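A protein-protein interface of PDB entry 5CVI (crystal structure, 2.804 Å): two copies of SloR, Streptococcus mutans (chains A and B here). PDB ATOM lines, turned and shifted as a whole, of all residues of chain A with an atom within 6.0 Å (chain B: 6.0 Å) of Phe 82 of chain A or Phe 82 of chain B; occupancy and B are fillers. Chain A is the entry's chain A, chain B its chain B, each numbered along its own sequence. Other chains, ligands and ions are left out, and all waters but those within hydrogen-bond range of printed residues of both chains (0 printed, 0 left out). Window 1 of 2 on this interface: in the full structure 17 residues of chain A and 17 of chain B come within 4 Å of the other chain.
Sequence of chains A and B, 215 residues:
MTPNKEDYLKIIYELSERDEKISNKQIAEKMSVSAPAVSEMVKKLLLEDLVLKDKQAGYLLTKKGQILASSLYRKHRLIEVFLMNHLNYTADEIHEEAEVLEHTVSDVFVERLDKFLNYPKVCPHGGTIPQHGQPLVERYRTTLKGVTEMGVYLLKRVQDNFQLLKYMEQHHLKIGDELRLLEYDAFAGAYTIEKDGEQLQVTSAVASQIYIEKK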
ATOM      1  N   ARG A  77     -13.713  -7.510  17.324  1.00  0.00           N
ATOM      2  CA  ARG A  77     -13.448  -8.892  16.945  1.00  0.00           C
ATOM      3  C   ARG A  77     -14.687  -9.792  16.974  1.00  0.00           C
ATOM      4  O   ARG A  77     -14.861 -10.634  16.092  1.00  0.00           O
ATOM      5  CB  ARG A  77     -12.302  -9.471  17.778  1.00  0.00           C
ATOM      6  CG  ARG A  77     -10.952  -8.859  17.424  1.00  0.00           C
ATOM      7  CD  ARG A  77      -9.819  -9.395  18.286  1.00  0.00           C
ATOM      8  NE  ARG A  77      -8.523  -8.901  17.824  1.00  0.00           N
ATOM      9  CZ  ARG A  77      -7.425  -8.861  18.572  1.00  0.00           C
ATOM     10  NH1 ARG A  77      -7.456  -9.283  19.828  1.00  0.00           N
ATOM     11  NH2 ARG A  77      -6.296  -8.392  18.063  1.00  0.00           N
ATOM     12  N   LEU A  78     -15.551  -9.616  17.971  1.00  0.00           N
ATOM     13  CA  LEU A  78     -16.816 -10.350  17.996  1.00  0.00           C
ATOM     14  C   LEU A  78     -17.650 -10.013  16.762  1.00  0.00           C
ATOM     15  O   LEU A  78     -18.264 -10.887  16.157  1.00  0.00           O
ATOM     16  CB  LEU A  78     -17.599 -10.056  19.274  1.00  0.00           C
ATOM     17  CG  LEU A  78     -17.161 -10.856  20.502  1.00  0.00           C
ATOM     18  CD1 LEU A  78     -17.836 -10.338  21.762  1.00  0.00           C
ATOM     19  CD2 LEU A  78     -17.467 -12.330  20.302  1.00  0.00           C
ATOM     20  N   ILE A  79     -17.643  -8.741  16.379  1.00  0.00           N
ATOM     21  CA  ILE A  79     -18.321  -8.298  15.167  1.00  0.00           C
ATOM     22  C   ILE A  79     -17.704  -8.920  13.919  1.00  0.00           C
ATOM     23  O   ILE A  79     -18.414  -9.231  12.963  1.00  0.00           O
ATOM     24  CB  ILE A  79     -18.305  -6.761  15.034  1.00  0.00           C
ATOM     25  CG1 ILE A  79     -19.044  -6.115  16.210  1.00  0.00           C
ATOM     26  CG2 ILE A  79     -18.925  -6.329  13.708  1.00  0.00           C
ATOM     27  CD1 ILE A  79     -18.969  -4.603  16.230  1.00  0.00           C
ATOM     28  N   GLU A  80     -16.385  -9.100  13.927  1.00  0.00           N
ATOM     29  CA  GLU A  80     -15.702  -9.702  12.784  1.00  0.00           C
ATOM     30  C   GLU A  80     -16.108 -11.163  12.594  1.00  0.00           C
ATOM     31  O   GLU A  80     -16.347 -11.608  11.472  1.00  0.00           O
ATOM     32  CB  GLU A  80     -14.182  -9.587  12.923  1.00  0.00           C
ATOM     33  CG  GLU A  80     -13.623  -8.201  12.667  1.00  0.00           C
ATOM     34  CD  GLU A  80     -12.109  -8.159  12.789  1.00  0.00           C
ATOM     35  OE1 GLU A  80     -11.495  -7.179  12.311  1.00  0.00           O
ATOM     36  OE2 GLU A  80     -11.535  -9.111  13.365  1.00  0.00           O
ATOM     37  N   VAL A  81     -16.190 -11.905  13.695  1.00  0.00           N
ATOM     38  CA  VAL A  81     -16.603 -13.303  13.640  1.00  0.00           C
ATOM     39  C   VAL A  81     -18.019 -13.442  13.089  1.00  0.00           C
ATOM     40  O   VAL A  81     -18.303 -14.357  12.316  1.00  0.00           O
ATOM     41  CB  VAL A  81     -16.549 -13.974  15.024  1.00  0.00           C
ATOM     42  CG1 VAL A  81     -17.046 -15.409  14.933  1.00  0.00           C
ATOM     43  CG2 VAL A  81     -15.141 -13.930  15.583  1.00  0.00           C
ATOM     44  N   PHE A  82     -18.904 -12.534  13.488  1.00  0.00           N
ATOM     45  CA  PHE A  82     -20.286 -12.575  13.022  1.00  0.00           C
ATOM     46  C   PHE A  82     -20.404 -12.231  11.542  1.00  0.00           C
ATOM     47  O   PHE A  82     -21.117 -12.905  10.795  1.00  0.00           O
ATOM     48  CB  PHE A  82     -21.178 -11.632  13.832  1.00  0.00           C
ATOM     49  CG  PHE A  82     -22.599 -11.589  13.345  1.00  0.00           C
ATOM     50  CD1 PHE A  82     -23.487 -12.602  13.675  1.00  0.00           C
ATOM     51  CD2 PHE A  82     -23.044 -10.548  12.545  1.00  0.00           C
ATOM     52  CE1 PHE A  82     -24.796 -12.572  13.223  1.00  0.00           C
ATOM     53  CE2 PHE A  82     -24.348 -10.513  12.091  1.00  0.00           C
ATOM     54  CZ  PHE A  82     -25.227 -11.526  12.430  1.00  0.00           C
ATOM     55  N   LEU A  83     -19.718 -11.169  11.131  1.00  0.00           N
ATOM     56  CA  LEU A  83     -19.795 -10.699   9.756  1.00  0.00           C
ATOM     57  C   LEU A  83     -19.289 -11.749   8.776  1.00  0.00           C
ATOM     58  O   LEU A  83     -19.824 -11.899   7.682  1.00  0.00           O
ATOM     59  CB  LEU A  83     -18.999  -9.405   9.582  1.00  0.00           C
ATOM     60  CG  LEU A  83     -19.581  -8.121  10.173  1.00  0.00           C
ATOM     61  CD1 LEU A  83     -18.649  -6.944   9.906  1.00  0.00           C
ATOM     62  CD2 LEU A  83     -20.965  -7.844   9.596  1.00  0.00           C
ATOM     63  N   MET A  84     -18.255 -12.477   9.175  1.00  0.00           N
ATOM     64  CA  MET A  84     -17.606 -13.408   8.263  1.00  0.00           C
ATOM     65  C   MET A  84     -18.249 -14.788   8.255  1.00  0.00           C
ATOM     66  O   MET A  84     -18.498 -15.356   7.192  1.00  0.00           O
ATOM     67  CB  MET A  84     -16.115 -13.523   8.580  1.00  0.00           C
ATOM     68  CG  MET A  84     -15.353 -14.356   7.564  1.00  0.00           C
ATOM     69  SD  MET A  84     -13.446 -13.991   7.550  1.00  0.00           S
ATOM     70  CE  MET A  84     -13.519 -12.048   7.432  1.00  0.00           C
ATOM     71  N   ASN A  85     -18.520 -15.325   9.440  1.00  0.00           N
ATOM     72  CA  ASN A  85     -19.049 -16.678   9.553  1.00  0.00           C
ATOM     73  C   ASN A  85     -20.559 -16.771   9.349  1.00  0.00           C
ATOM     74  O   ASN A  85     -21.080 -17.836   9.023  1.00  0.00           O
ATOM     75  CB  ASN A  85     -18.659 -17.298  10.898  1.00  0.00           C
ATOM     76  CG  ASN A  85     -17.165 -17.514  11.027  1.00  0.00           C
ATOM     77  OD1 ASN A  85     -16.464 -17.700  10.033  1.00  0.00           O
ATOM     78  ND2 ASN A  85     -16.668 -17.493  12.261  1.00  0.00           N
ATOM     79  N   HIS A  86     -21.255 -15.654   9.534  1.00  0.00           N
ATOM     80  CA  HIS A  86     -22.714 -15.647   9.469  1.00  0.00           C
ATOM     81  C   HIS A  86     -23.287 -14.766   8.353  1.00  0.00           C
ATOM     82  O   HIS A  86     -24.307 -15.107   7.756  1.00  0.00           O
ATOM     83  CB  HIS A  86     -23.312 -15.255  10.827  1.00  0.00           C
ATOM     84  CG  HIS A  86     -23.028 -16.240  11.920  1.00  0.00           C
ATOM     85  ND1 HIS A  86     -23.932 -17.205  12.305  1.00  0.00           N
ATOM     86  CD2 HIS A  86     -21.939 -16.406  12.709  1.00  0.00           C
ATOM     87  CE1 HIS A  86     -23.415 -17.925  13.287  1.00  0.00           C
ATOM     88  NE2 HIS A  86     -22.206 -17.460  13.549  1.00  0.00           N
ATOM     89  N   LEU A  87     -22.642 -13.638   8.073  1.00  0.00           N
ATOM     90  CA  LEU A  87     -23.090 -12.774   6.981  1.00  0.00           C
ATOM     91  C   LEU A  87     -22.201 -12.926   5.751  1.00  0.00           C
ATOM     92  O   LEU A  87     -22.387 -12.235   4.749  1.00  0.00           O
ATOM     93  CB  LEU A  87     -23.177 -11.309   7.421  1.00  0.00           C
ATOM     94  CG  LEU A  87     -24.320 -10.986   8.390  1.00  0.00           C
ATOM     95  CD1 LEU A  87     -24.396  -9.496   8.710  1.00  0.00           C
ATOM     96  CD2 LEU A  87     -25.648 -11.477   7.826  1.00  0.00           C
ATOM     97  N   ASN A  88     -21.239 -13.840   5.839  1.00  0.00           N
ATOM     98  CA  ASN A  88     -20.371 -14.176   4.710  1.00  0.00           C
ATOM     99  C   ASN A  88     -19.577 -12.998   4.146  1.00  0.00           C
ATOM    100  O   ASN A  88     -19.407 -12.879   2.934  1.00  0.00           O
ATOM    101  CB  ASN A  88     -21.175 -14.858   3.599  1.00  0.00           C
ATOM    102  CG  ASN A  88     -21.826 -16.145   4.058  1.00  0.00           C
ATOM    103  OD1 ASN A  88     -21.247 -16.906   4.839  1.00  0.00           O
ATOM    104  ND2 ASN A  88     -23.045 -16.393   3.582  1.00  0.00           N
ATOM    105  N   PHE A 109     -25.667  -5.857  23.598  1.00  0.00           N
ATOM    106  CA  PHE A 109     -25.519  -6.417  22.259  1.00  0.00           C
ATOM    107  C   PHE A 109     -24.245  -7.240  22.169  1.00  0.00           C
ATOM    108  O   PHE A 109     -24.260  -8.379  21.689  1.00  0.00           O
ATOM    109  CB  PHE A 109     -25.477  -5.310  21.206  1.00  0.00           C
ATOM    110  CG  PHE A 109     -25.352  -5.820  19.794  1.00  0.00           C
ATOM    111  CD1 PHE A 109     -24.106  -6.053  19.229  1.00  0.00           C
ATOM    112  CD2 PHE A 109     -26.483  -6.058  19.030  1.00  0.00           C
ATOM    113  CE1 PHE A 109     -23.994  -6.520  17.928  1.00  0.00           C
ATOM    114  CE2 PHE A 109     -26.375  -6.526  17.735  1.00  0.00           C
ATOM    115  CZ  PHE A 109     -25.132  -6.754  17.184  1.00  0.00           C
ATOM    116  N   LEU A 113     -24.237 -11.263  21.554  1.00  0.00           N
ATOM    117  CA  LEU A 113     -23.630 -11.773  20.336  1.00  0.00           C
ATOM    118  C   LEU A 113     -22.532 -12.764  20.698  1.00  0.00           C
ATOM    119  O   LEU A 113     -22.322 -13.753  19.999  1.00  0.00           O
ATOM    120  CB  LEU A 113     -23.051 -10.636  19.495  1.00  0.00           C
ATOM    121  CG  LEU A 113     -22.367 -11.072  18.196  1.00  0.00           C
ATOM    122  CD1 LEU A 113     -23.373 -11.680  17.227  1.00  0.00           C
ATOM    123  CD2 LEU A 113     -21.626  -9.910  17.544  1.00  0.00           C
ATOM    124  N   PHE A 116     -24.201 -15.975  21.406  1.00  0.00           N
ATOM    125  CA  PHE A 116     -24.739 -16.475  20.145  1.00  0.00           C
ATOM    126  C   PHE A 116     -23.662 -17.136  19.286  1.00  0.00           C
ATOM    127  O   PHE A 116     -23.908 -18.160  18.648  1.00  0.00           O
ATOM    128  CB  PHE A 116     -25.413 -15.336  19.377  1.00  0.00           C
ATOM    129  CG  PHE A 116     -25.693 -15.655  17.943  1.00  0.00           C
ATOM    130  CD1 PHE A 116     -26.841 -16.340  17.581  1.00  0.00           C
ATOM    131  CD2 PHE A 116     -24.809 -15.266  16.953  1.00  0.00           C
ATOM    132  CE1 PHE A 116     -27.097 -16.634  16.259  1.00  0.00           C
ATOM    133  CE2 PHE A 116     -25.060 -15.556  15.631  1.00  0.00           C
ATOM    134  CZ  PHE A 116     -26.204 -16.240  15.281  1.00  0.00           C
ATOM    135  N   LEU A 117     -22.472 -16.544  19.283  1.00  0.00           N
ATOM    136  CA  LEU A 117     -21.347 -17.060  18.513  1.00  0.00           C
ATOM    137  C   LEU A 117     -20.661 -18.214  19.235  1.00  0.00           C
ATOM    138  O   LEU A 117     -19.677 -18.769  18.746  1.00  0.00           O
ATOM    139  CB  LEU A 117     -20.335 -15.945  18.252  1.00  0.00           C
ATOM    140  CG  LEU A 117     -20.826 -14.752  17.437  1.00  0.00           C
ATOM    141  CD1 LEU A 117     -19.744 -13.689  17.353  1.00  0.00           C
ATOM    142  CD2 LEU A 117     -21.232 -15.209  16.042  1.00  0.00           C
ATOM    143  N   ARG B  77     -37.118  -2.952  11.142  1.00  0.00           N
ATOM    144  CA  ARG B  77     -37.843  -4.199  11.353  1.00  0.00           C
ATOM    145  C   ARG B  77     -36.974  -5.425  11.079  1.00  0.00           C
ATOM    146  O   ARG B  77     -37.118  -6.458  11.730  1.00  0.00           O
ATOM    147  CB  ARG B  77     -39.125  -4.226  10.512  1.00  0.00           C
ATOM    148  CG  ARG B  77     -40.193  -3.258  11.011  1.00  0.00           C
ATOM    149  CD  ARG B  77     -41.432  -3.231  10.130  1.00  0.00           C
ATOM    150  NE  ARG B  77     -42.403  -2.251  10.614  1.00  0.00           N
ATOM    151  CZ  ARG B  77     -43.454  -1.823   9.919  1.00  0.00           C
ATOM    152  NH1 ARG B  77     -43.683  -2.289   8.697  1.00  0.00           N
ATOM    153  NH2 ARG B  77     -44.275  -0.921  10.445  1.00  0.00           N
ATOM    154  N   LEU B  78     -36.068  -5.305  10.117  1.00  0.00           N
ATOM    155  CA  LEU B  78     -35.128  -6.378   9.827  1.00  0.00           C
ATOM    156  C   LEU B  78     -34.182  -6.571  11.010  1.00  0.00           C
ATOM    157  O   LEU B  78     -33.798  -7.695  11.330  1.00  0.00           O
ATOM    158  CB  LEU B  78     -34.344  -6.070   8.550  1.00  0.00           C
ATOM    159  CG  LEU B  78     -34.342  -7.128   7.445  1.00  0.00           C
ATOM    160  CD1 LEU B  78     -35.681  -7.831   7.371  1.00  0.00           C
ATOM    161  CD2 LEU B  78     -34.016  -6.480   6.106  1.00  0.00           C
ATOM    162  N   ILE B  79     -33.822  -5.473  11.669  1.00  0.00           N
ATOM    163  CA  ILE B  79     -32.912  -5.522  12.811  1.00  0.00           C
ATOM    164  C   ILE B  79     -33.560  -6.102  14.061  1.00  0.00           C
ATOM    165  O   ILE B  79     -32.910  -6.825  14.820  1.00  0.00           O
ATOM    166  CB  ILE B  79     -32.343  -4.130  13.156  1.00  0.00           C
ATOM    167  CG1 ILE B  79     -31.358  -3.669  12.081  1.00  0.00           C
ATOM    168  CG2 ILE B  79     -31.652  -4.155  14.511  1.00  0.00           C
ATOM    169  CD1 ILE B  79     -30.855  -2.257  12.287  1.00  0.00           C
ATOM    170  N   GLU B  80     -34.831  -5.784  14.284  1.00  0.00           N
ATOM    171  CA  GLU B  80     -35.499  -6.270  15.486  1.00  0.00           C
ATOM    172  C   GLU B  80     -35.945  -7.728  15.341  1.00  0.00           C
ATOM    173  O   GLU B  80     -36.187  -8.409  16.331  1.00  0.00           O
ATOM    174  CB  GLU B  80     -36.654  -5.353  15.902  1.00  0.00           C
ATOM    175  CG  GLU B  80     -37.740  -5.189  14.861  1.00  0.00           C
ATOM    176  CD  GLU B  80     -38.856  -4.264  15.319  1.00  0.00           C
ATOM    177  OE1 GLU B  80     -38.610  -3.400  16.190  1.00  0.00           O
ATOM    178  OE2 GLU B  80     -39.987  -4.405  14.809  1.00  0.00           O
ATOM    179  N   VAL B  81     -36.045  -8.204  14.105  1.00  0.00           N
ATOM    180  CA  VAL B  81     -36.280  -9.624  13.868  1.00  0.00           C
ATOM    181  C   VAL B  81     -35.050 -10.419  14.288  1.00  0.00           C
ATOM    182  O   VAL B  81     -35.168 -11.505  14.855  1.00  0.00           O
ATOM    183  CB  VAL B  81     -36.581  -9.932  12.387  1.00  0.00           C
ATOM    184  CG1 VAL B  81     -36.520 -11.434  12.139  1.00  0.00           C
ATOM    185  CG2 VAL B  81     -37.935  -9.379  11.987  1.00  0.00           C
ATOM    186  N   PHE B  82     -33.873  -9.868  14.002  1.00  0.00           N
ATOM    187  CA  PHE B  82     -32.605 -10.508  14.342  1.00  0.00           C
ATOM    188  C   PHE B  82     -32.348 -10.450  15.845  1.00  0.00           C
ATOM    189  O   PHE B  82     -31.923 -11.431  16.456  1.00  0.00           O
ATOM    190  CB  PHE B  82     -31.453  -9.846  13.575  1.00  0.00           C
ATOM    191  CG  PHE B  82     -30.083 -10.243  14.058  1.00  0.00           C
ATOM    192  CD1 PHE B  82     -29.605 -11.530  13.864  1.00  0.00           C
ATOM    193  CD2 PHE B  82     -29.263  -9.320  14.685  1.00  0.00           C
ATOM    194  CE1 PHE B  82     -28.343 -11.886  14.302  1.00  0.00           C
ATOM    195  CE2 PHE B  82     -28.006  -9.671  15.119  1.00  0.00           C
ATOM    196  CZ  PHE B  82     -27.544 -10.955  14.928  1.00  0.00           C
ATOM    197  N   LEU B  83     -32.613  -9.290  16.433  1.00  0.00           N
ATOM    198  CA  LEU B  83     -32.359  -9.079  17.851  1.00  0.00           C
ATOM    199  C   LEU B  83     -33.207  -9.997  18.718  1.00  0.00           C
ATOM    200  O   LEU B  83     -32.767 -10.463  19.761  1.00  0.00           O
ATOM    201  CB  LEU B  83     -32.614  -7.615  18.222  1.00  0.00           C
ATOM    202  CG  LEU B  83     -31.689  -6.580  17.581  1.00  0.00           C
ATOM    203  CD1 LEU B  83     -32.047  -5.178  18.051  1.00  0.00           C
ATOM    204  CD2 LEU B  83     -30.235  -6.895  17.899  1.00  0.00           C
ATOM    205  N   MET B  84     -34.430 -10.253  18.270  1.00  0.00           N
ATOM    206  CA  MET B  84     -35.386 -11.040  19.038  1.00  0.00           C
ATOM    207  C   MET B  84     -35.223 -12.539  18.794  1.00  0.00           C
ATOM    208  O   MET B  84     -35.205 -13.334  19.734  1.00  0.00           O
ATOM    209  CB  MET B  84     -36.812 -10.590  18.707  1.00  0.00           C
ATOM    210  CG  MET B  84     -37.912 -11.378  19.399  1.00  0.00           C
ATOM    211  SD  MET B  84     -39.637 -10.452  19.325  1.00  0.00           S
ATOM    212  CE  MET B  84     -39.205  -8.947  20.474  1.00  0.00           C
ATOM    213  N   ASN B  85     -35.082 -12.916  17.529  1.00  0.00           N
ATOM    214  CA  ASN B  85     -35.037 -14.324  17.149  1.00  0.00           C
ATOM    215  C   ASN B  85     -33.661 -14.975  17.290  1.00  0.00           C
ATOM    216  O   ASN B  85     -33.555 -16.199  17.370  1.00  0.00           O
ATOM    217  CB  ASN B  85     -35.557 -14.507  15.718  1.00  0.00           C
ATOM    218  CG  ASN B  85     -37.071 -14.580  15.652  1.00  0.00           C
ATOM    219  OD1 ASN B  85     -37.764 -13.563  15.748  1.00  0.00           O
ATOM    220  ND2 ASN B  85     -37.594 -15.791  15.481  1.00  0.00           N
ATOM    221  N   HIS B  86     -32.614 -14.156  17.325  1.00  0.00           N
ATOM    222  CA  HIS B  86     -31.246 -14.668  17.340  1.00  0.00           C
ATOM    223  C   HIS B  86     -30.461 -14.240  18.575  1.00  0.00           C
ATOM    224  O   HIS B  86     -29.789 -15.058  19.200  1.00  0.00           O
ATOM    225  CB  HIS B  86     -30.499 -14.242  16.072  1.00  0.00           C
ATOM    226  CG  HIS B  86     -31.036 -14.856  14.818  1.00  0.00           C
ATOM    227  ND1 HIS B  86     -30.549 -16.036  14.300  1.00  0.00           N
ATOM    228  CD2 HIS B  86     -32.021 -14.455  13.981  1.00  0.00           C
ATOM    229  CE1 HIS B  86     -31.208 -16.335  13.196  1.00  0.00           C
ATOM    230  NE2 HIS B  86     -32.108 -15.392  12.981  1.00  0.00           N
ATOM    231  N   LEU B  87     -30.537 -12.957  18.915  1.00  0.00           N
ATOM    232  CA  LEU B  87     -29.810 -12.437  20.068  1.00  0.00           C
ATOM    233  C   LEU B  87     -30.655 -12.476  21.338  1.00  0.00           C
ATOM    234  O   LEU B  87     -30.195 -12.088  22.413  1.00  0.00           O
ATOM    235  CB  LEU B  87     -29.283 -11.024  19.807  1.00  0.00           C
ATOM    236  CG  LEU B  87     -28.179 -10.920  18.754  1.00  0.00           C
ATOM    237  CD1 LEU B  87     -27.438  -9.590  18.866  1.00  0.00           C
ATOM    238  CD2 LEU B  87     -27.208 -12.082  18.878  1.00  0.00           C
ATOM    239  N   ASN B  88     -31.894 -12.936  21.202  1.00  0.00           N
ATOM    240  CA  ASN B  88     -32.753 -13.178  22.356  1.00  0.00           C
ATOM    241  C   ASN B  88     -33.160 -11.915  23.107  1.00  0.00           C
ATOM    242  O   ASN B  88     -33.305 -11.930  24.327  1.00  0.00           O
ATOM    243  CB  ASN B  88     -32.084 -14.166  23.310  1.00  0.00           C
ATOM    244  CG  ASN B  88     -31.656 -15.438  22.617  1.00  0.00           C
ATOM    245  OD1 ASN B  88     -32.433 -16.047  21.879  1.00  0.00           O
ATOM    246  ND2 ASN B  88     -30.406 -15.838  22.831  1.00  0.00           N
ATOM    247  N   PHE B 109     -24.796  -4.684   4.655  1.00  0.00           N
ATOM    248  CA  PHE B 109     -25.141  -5.337   5.912  1.00  0.00           C
ATOM    249  C   PHE B 109     -26.626  -5.657   5.923  1.00  0.00           C
ATOM    250  O   PHE B 109     -27.027  -6.798   6.143  1.00  0.00           O
ATOM    251  CB  PHE B 109     -24.797  -4.443   7.104  1.00  0.00           C
ATOM    252  CG  PHE B 109     -25.047  -5.091   8.437  1.00  0.00           C
ATOM    253  CD1 PHE B 109     -24.033  -5.762   9.093  1.00  0.00           C
ATOM    254  CD2 PHE B 109     -26.298  -5.030   9.031  1.00  0.00           C
ATOM    255  CE1 PHE B 109     -24.259  -6.357  10.317  1.00  0.00           C
ATOM    256  CE2 PHE B 109     -26.529  -5.622  10.252  1.00  0.00           C
ATOM    257  CZ  PHE B 109     -25.507  -6.287  10.898  1.00  0.00           C
ATOM    258  N   LEU B 113     -28.125  -9.359   5.774  1.00  0.00           N
ATOM    259  CA  LEU B 113     -28.851  -9.831   6.948  1.00  0.00           C
ATOM    260  C   LEU B 113     -30.235 -10.331   6.549  1.00  0.00           C
ATOM    261  O   LEU B 113     -30.771 -11.255   7.158  1.00  0.00           O
ATOM    262  CB  LEU B 113     -28.982  -8.723   7.993  1.00  0.00           C
ATOM    263  CG  LEU B 113     -29.921  -9.059   9.156  1.00  0.00           C
ATOM    264  CD1 LEU B 113     -29.366 -10.209   9.979  1.00  0.00           C
ATOM    265  CD2 LEU B 113     -30.175  -7.843  10.035  1.00  0.00           C
ATOM    266  N   PHE B 116     -29.777 -13.662   5.451  1.00  0.00           N
ATOM    267  CA  PHE B 116     -29.481 -14.412   6.664  1.00  0.00           C
ATOM    268  C   PHE B 116     -30.755 -14.824   7.400  1.00  0.00           C
ATOM    269  O   PHE B 116     -30.861 -15.946   7.893  1.00  0.00           O
ATOM    270  CB  PHE B 116     -28.578 -13.592   7.587  1.00  0.00           C
ATOM    271  CG  PHE B 116     -28.358 -14.219   8.930  1.00  0.00           C
ATOM    272  CD1 PHE B 116     -27.435 -15.235   9.092  1.00  0.00           C
ATOM    273  CD2 PHE B 116     -29.075 -13.787  10.034  1.00  0.00           C
ATOM    274  CE1 PHE B 116     -27.232 -15.813  10.328  1.00  0.00           C
ATOM    275  CE2 PHE B 116     -28.875 -14.361  11.274  1.00  0.00           C
ATOM    276  CZ  PHE B 116     -27.952 -15.375  11.421  1.00  0.00           C
ATOM    277  N   LEU B 117     -31.718 -13.910   7.467  1.00  0.00           N
ATOM    278  CA  LEU B 117     -32.984 -14.168   8.145  1.00  0.00           C
ATOM    279  C   LEU B 117     -33.977 -14.880   7.227  1.00  0.00           C
ATOM    280  O   LEU B 117     -35.147 -15.058   7.578  1.00  0.00           O
ATOM    281  CB  LEU B 117     -33.591 -12.858   8.660  1.00  0.00           C
ATOM    282  CG  LEU B 117     -32.796 -12.122   9.740  1.00  0.00           C
ATOM    283  CD1 LEU B 117     -33.372 -10.733   9.991  1.00  0.00           C
ATOM    284  CD2 LEU B 117     -32.779 -12.933  11.027  1.00  0.00           C
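The backbone carbonyl oxygen of Phe 82 of chain A is in hydrogen-bond range of the backbone NH of Leu 87 of chain A (3.2 Å).
O of Leu 83 of chain A is in hydrogen-bond range of N of Asn 88 of chain A (3.0 Å).
The backbone carbonyl oxygen of Phe 82 of chain B lies within hydrogen-bond range of the backbone NH of Leu 87 of chain B, at 3.2 Å.
N of Asn 88 of chain B sits at hydrogen-bond distance from O of Leu 83 of chain B (3.0 Å).
Printed residues of chain B within 4 Å of Phe 82 of chain A: Phe 82.
Phe 82 of chain B touches just one residue of chain A: Phe 82.
Of the printed residues of chain A, Phe 109 of chain B touches Leu 83 (3.7 Å) and Leu 87 (3.5 Å).
Of the printed residues of chain A, Phe 116 of chain B touches His 86 (3.4 Å) and Leu 87 (3.6 Å).
Printed residues of chain B within 4 Å of Leu 83 of chain A: Phe 109 (3.7 Å).
Of the printed residues of chain B, Phe 109 of chain A touches Leu 83 and Leu 87.
Leu 78 of chain A touches none of the printed residues of chain B.
The nearest residue of chain A that does not touch Phe 82 of chain B is Phe 109 of chain A (4.4 Å).
Of the 16 printed residues of chain B, 7 touch a printed residue of chain A.
Of the 16 printed residues of chain A, 7 touch a printed residue of chain B.
Among the printed residues, no Asp or Glu carboxylate lies within 4 Å of a Lys or Arg side-chain nitrogen of the other chain.
Among the printed residues, pairs that only touch across the chains: Phe 82 of chain A with Phe 82 of chain B, Leu 83 of chain A with Phe 109 of chain B, His 86 of chain A with Phe 116 of chain B, Leu 87 of chain A with Phe 109 of chain B, Leu 87 of chain A with Leu 113 of chain B, Leu 87 of chain A with Phe 116 of chain B, Phe 109 of chain A with Leu 83 of chain B, Phe 109 of chain A with Leu 87 of chain B, Leu 113 of chain A with Leu 87 of chain B, Phe 116 of chain A with His 86 of chain B and Phe 116 of chain A with Leu 87 of chain B.
Phe 82 of chain A touches its own counterpart, Phe 82 of chain B.
Leu 83 of chain A touches Phe 109 of chain B, and with the chains exchanged Phe 109 of chain A touches Leu 83 of chain B.
His 86 of chain A touches Phe 116 of chain B, and with the chains exchanged Phe 116 of chain A touches His 86 of chain B.
Leu 87 of chain A touches Leu 113 of chain B, and with the chains exchanged Leu 113 of chain A touches Leu 87 of chain B.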
